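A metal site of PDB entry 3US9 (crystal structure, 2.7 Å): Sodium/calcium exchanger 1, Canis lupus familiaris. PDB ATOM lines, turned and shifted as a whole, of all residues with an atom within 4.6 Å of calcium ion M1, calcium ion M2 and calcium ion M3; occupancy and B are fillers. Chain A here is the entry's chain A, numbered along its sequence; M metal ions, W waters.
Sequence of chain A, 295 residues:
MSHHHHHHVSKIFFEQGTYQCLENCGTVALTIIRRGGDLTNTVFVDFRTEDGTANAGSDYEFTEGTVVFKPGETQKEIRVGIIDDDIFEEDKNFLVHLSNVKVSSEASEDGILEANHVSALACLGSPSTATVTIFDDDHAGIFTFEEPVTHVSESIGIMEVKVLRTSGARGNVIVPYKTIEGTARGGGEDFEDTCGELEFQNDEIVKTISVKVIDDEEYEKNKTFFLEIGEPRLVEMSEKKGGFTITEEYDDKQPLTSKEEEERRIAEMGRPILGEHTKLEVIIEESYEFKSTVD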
ATOM      1  N   GLU A  23     -25.647  12.649 -17.448  1.00  0.00           N
ATOM      2  CA  GLU A  23     -25.167  12.301 -18.778  1.00  0.00           C
ATOM      3  C   GLU A  23     -26.299  12.190 -19.792  1.00  0.00           C
ATOM      4  O   GLU A  23     -26.102  12.455 -20.980  1.00  0.00           O
ATOM      5  CB  GLU A  23     -24.373  10.998 -18.741  1.00  0.00           C
ATOM      6  CG  GLU A  23     -23.627  10.735 -20.027  1.00  0.00           C
ATOM      7  CD  GLU A  23     -22.984   9.367 -20.046  1.00  0.00           C
ATOM      8  OE1 GLU A  23     -23.245   8.593 -20.996  1.00  0.00           O
ATOM      9  OE2 GLU A  23     -22.209   9.080 -19.115  1.00  0.00           O
ATOM     10  N   ASP A  59     -17.596  12.714 -24.193  1.00  0.00           N
ATOM     11  CA  ASP A  59     -18.342  13.077 -22.990  1.00  0.00           C
ATOM     12  C   ASP A  59     -19.337  14.186 -23.259  1.00  0.00           C
ATOM     13  O   ASP A  59     -20.314  14.343 -22.532  1.00  0.00           O
ATOM     14  CB  ASP A  59     -17.383  13.481 -21.864  1.00  0.00           C
ATOM     15  CG  ASP A  59     -16.428  12.367 -21.472  1.00  0.00           C
ATOM     16  OD1 ASP A  59     -16.835  11.512 -20.663  1.00  0.00           O
ATOM     17  OD2 ASP A  59     -15.290  12.358 -21.974  1.00  0.00           O
ATOM     18  N   ILE A  83     -23.153  14.140 -24.494  1.00  0.00           N
ATOM     19  CA  ILE A  83     -23.165  12.826 -25.134  1.00  0.00           C
ATOM     20  C   ILE A  83     -23.411  11.705 -24.138  1.00  0.00           C
ATOM     21  O   ILE A  83     -22.760  11.619 -23.095  1.00  0.00           O
ATOM     22  CB  ILE A  83     -21.864  12.548 -25.907  1.00  0.00           C
ATOM     23  CG1 ILE A  83     -21.676  13.579 -27.027  1.00  0.00           C
ATOM     24  CG2 ILE A  83     -21.878  11.148 -26.482  1.00  0.00           C
ATOM     25  CD1 ILE A  83     -20.454  13.346 -27.875  1.00  0.00           C
ATOM     26  N   ASP A  84     -24.363  10.848 -24.472  1.00  0.00           N
ATOM     27  CA  ASP A  84     -24.724   9.744 -23.611  1.00  0.00           C
ATOM     28  C   ASP A  84     -24.449   8.375 -24.245  1.00  0.00           C
ATOM     29  O   ASP A  84     -24.793   8.138 -25.406  1.00  0.00           O
ATOM     30  CB  ASP A  84     -26.208   9.845 -23.259  1.00  0.00           C
ATOM     31  CG  ASP A  84     -26.648   8.785 -22.289  1.00  0.00           C
ATOM     32  OD1 ASP A  84     -25.766   8.192 -21.649  1.00  0.00           O
ATOM     33  OD2 ASP A  84     -27.871   8.561 -22.168  1.00  0.00           O
ATOM     34  N   ASP A  85     -23.833   7.485 -23.464  1.00  0.00           N
ATOM     35  CA  ASP A  85     -23.657   6.089 -23.843  1.00  0.00           C
ATOM     36  C   ASP A  85     -24.008   5.216 -22.632  1.00  0.00           C
ATOM     37  O   ASP A  85     -24.538   5.720 -21.666  1.00  0.00           O
ATOM     38  CB  ASP A  85     -22.231   5.828 -24.331  1.00  0.00           C
ATOM     39  CG  ASP A  85     -21.179   6.322 -23.351  1.00  0.00           C
ATOM     40  OD1 ASP A  85     -21.484   6.440 -22.155  1.00  0.00           O
ATOM     41  OD2 ASP A  85     -20.033   6.584 -23.786  1.00  0.00           O
ATOM     42  N   ASP A  86     -23.718   3.924 -22.679  1.00  0.00           N
ATOM     43  CA  ASP A  86     -24.113   3.058 -21.568  1.00  0.00           C
ATOM     44  C   ASP A  86     -22.957   2.552 -20.700  1.00  0.00           C
ATOM     45  O   ASP A  86     -23.127   1.641 -19.889  1.00  0.00           O
ATOM     46  CB  ASP A  86     -24.949   1.873 -22.071  1.00  0.00           C
ATOM     47  CG  ASP A  86     -26.414   2.226 -22.244  1.00  0.00           C
ATOM     48  OD1 ASP A  86     -26.752   3.427 -22.207  1.00  0.00           O
ATOM     49  OD2 ASP A  86     -27.239   1.293 -22.405  1.00  0.00           O
ATOM     50  N   ILE A  87     -21.788   3.163 -20.866  1.00  0.00           N
ATOM     51  CA  ILE A  87     -20.576   2.693 -20.184  1.00  0.00           C
ATOM     52  C   ILE A  87     -20.282   3.462 -18.898  1.00  0.00           C
ATOM     53  O   ILE A  87     -19.858   4.617 -18.941  1.00  0.00           O
ATOM     54  CB  ILE A  87     -19.353   2.817 -21.106  1.00  0.00           C
ATOM     55  CG1 ILE A  87     -19.716   2.438 -22.545  1.00  0.00           C
ATOM     56  CG2 ILE A  87     -18.207   1.967 -20.585  1.00  0.00           C
ATOM     57  CD1 ILE A  87     -18.611   2.725 -23.545  1.00  0.00           C
ATOM     58  N   PHE A  88     -20.485   2.817 -17.751  1.00  0.00           N
ATOM     59  CA  PHE A  88     -20.246   3.456 -16.452  1.00  0.00           C
ATOM     60  C   PHE A  88     -18.944   4.259 -16.402  1.00  0.00           C
ATOM     61  O   PHE A  88     -17.880   3.761 -16.766  1.00  0.00           O
ATOM     62  CB  PHE A  88     -20.245   2.407 -15.336  1.00  0.00           C
ATOM     63  CG  PHE A  88     -20.029   2.988 -13.969  1.00  0.00           C
ATOM     64  CD1 PHE A  88     -21.021   3.728 -13.345  1.00  0.00           C
ATOM     65  CD2 PHE A  88     -18.839   2.780 -13.294  1.00  0.00           C
ATOM     66  CE1 PHE A  88     -20.824   4.263 -12.083  1.00  0.00           C
ATOM     67  CE2 PHE A  88     -18.639   3.307 -12.027  1.00  0.00           C
ATOM     68  CZ  PHE A  88     -19.625   4.049 -11.424  1.00  0.00           C
ATOM     69  N   GLU A  89     -19.036   5.498 -15.930  1.00  0.00           N
ATOM     70  CA  GLU A  89     -17.877   6.377 -15.796  1.00  0.00           C
ATOM     71  C   GLU A  89     -17.907   7.118 -14.460  1.00  0.00           C
ATOM     72  O   GLU A  89     -18.950   7.215 -13.824  1.00  0.00           O
ATOM     73  CB  GLU A  89     -17.870   7.415 -16.916  1.00  0.00           C
ATOM     74  CG  GLU A  89     -18.047   6.841 -18.298  1.00  0.00           C
ATOM     75  CD  GLU A  89     -18.528   7.881 -19.282  1.00  0.00           C
ATOM     76  OE1 GLU A  89     -17.693   8.608 -19.855  1.00  0.00           O
ATOM     77  OE2 GLU A  89     -19.753   7.972 -19.465  1.00  0.00           O
ATOM     78  N   ASP A 136     -22.481  10.646 -14.139  1.00  0.00           N
ATOM     79  CA  ASP A 136     -22.812   9.488 -14.948  1.00  0.00           C
ATOM     80  C   ASP A 136     -24.034   8.721 -14.444  1.00  0.00           C
ATOM     81  O   ASP A 136     -24.301   8.716 -13.230  1.00  0.00           O
ATOM     82  CB  ASP A 136     -21.625   8.545 -15.000  1.00  0.00           C
ATOM     83  CG  ASP A 136     -21.825   7.414 -15.984  1.00  0.00           C
ATOM     84  OD1 ASP A 136     -21.689   7.699 -17.178  1.00  0.00           O
ATOM     85  OD2 ASP A 136     -22.098   6.251 -15.571  1.00  0.00           O
ATOM     86  N   ASP A 137     -24.770   8.088 -15.347  1.00  0.00           N
ATOM     87  CA  ASP A 137     -26.004   7.410 -14.977  1.00  0.00           C
ATOM     88  C   ASP A 137     -26.041   5.966 -15.441  1.00  0.00           C
ATOM     89  O   ASP A 137     -27.096   5.459 -15.825  1.00  0.00           O
ATOM     90  CB  ASP A 137     -27.212   8.168 -15.539  1.00  0.00           C
ATOM     91  CG  ASP A 137     -27.267   8.135 -17.050  1.00  0.00           C
ATOM     92  OD1 ASP A 137     -28.314   8.501 -17.611  1.00  0.00           O
ATOM     93  OD2 ASP A 137     -26.263   7.737 -17.677  1.00  0.00           O
ATOM     94  N   ASP A 138     -24.909   5.283 -15.337  1.00  0.00           N
ATOM     95  CA  ASP A 138     -24.809   3.905 -15.816  1.00  0.00           C
ATOM     96  C   ASP A 138     -24.421   2.854 -14.762  1.00  0.00           C
ATOM     97  O   ASP A 138     -24.025   1.747 -15.138  1.00  0.00           O
ATOM     98  CB  ASP A 138     -23.848   3.834 -17.007  1.00  0.00           C
ATOM     99  CG  ASP A 138     -24.143   4.892 -18.057  1.00  0.00           C
ATOM    100  OD1 ASP A 138     -23.203   5.591 -18.486  1.00  0.00           O
ATOM    101  OD2 ASP A 138     -25.317   5.008 -18.461  1.00  0.00           O
HETATM  102 CA    CA M   1     -21.752   6.424 -19.400  1.00  0.00          CA
HETATM  103 CA    CA M   2     -19.983  10.418 -20.161  1.00  0.00          CA
HETATM  104 CA    CA M   3     -25.299   6.933 -19.617  1.00  0.00          CA
HETATM  105  O   HOH W   1     -20.040   9.140 -22.886  1.00  0.00           O
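OE1 of Glu 23 sits close to OD1 of Asp 84 (2.6 Å).
The backbone NH of Ile 83 is in hydrogen-bond range of the backbone carbonyl oxygen of Asp 59, at 3.5 Å.
Within 4 Å of calcium ion M1: Glu 23, Asp 85, Ile 87, Glu 89, Asp 136 and Asp 138.
The nearest printed residue that does not touch calcium ion M1 is Phe 88 (4.2 Å).
Asp 59 touches calcium ion M2.
Calcium ion M1 is bound by the side-chain carboxylate of Asp 138 (1.9 Å), the side-chain carboxylate of Glu 89 (2.5 Å), the side-chain carboxylate of Asp 136 (2.6 Å), the backbone carbonyl oxygen of Ile 87 (2.7 Å), the side-chain carboxylate of Glu 23 (2.7 Å) and the side-chain carboxylate of Asp 85 (2.8 Å).
Calcium ion M1 has six donor atoms within binding distance.
Slightly farther from calcium ion M1 lies OE1 of Glu 23 (3.1 Å).
Calcium ion M2 is bound by OE2 of Glu 89 (2.6 Å) and OE2 of Glu 23 (2.8 Å).
Calcium ion M2 has two donor atoms within binding distance.
Slightly farther from calcium ion M2 lies the side-chain carboxylate (OE1) of Glu 89 (2.9 Å).
Slightly farther from calcium ion M2 lies water W1 (3.0 Å).
Calcium ion M3 is bound by OD2 of Asp 138 (2.2 Å), OD2 of Asp 137 (2.3 Å), OD1 of Asp 84 (2.4 Å), O of Asp 85 (2.5 Å) and OD1 of Asp 138 (2.7 Å).
Slightly farther from calcium ion M3 lies OE1 of Glu 23 (3.0 Å).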
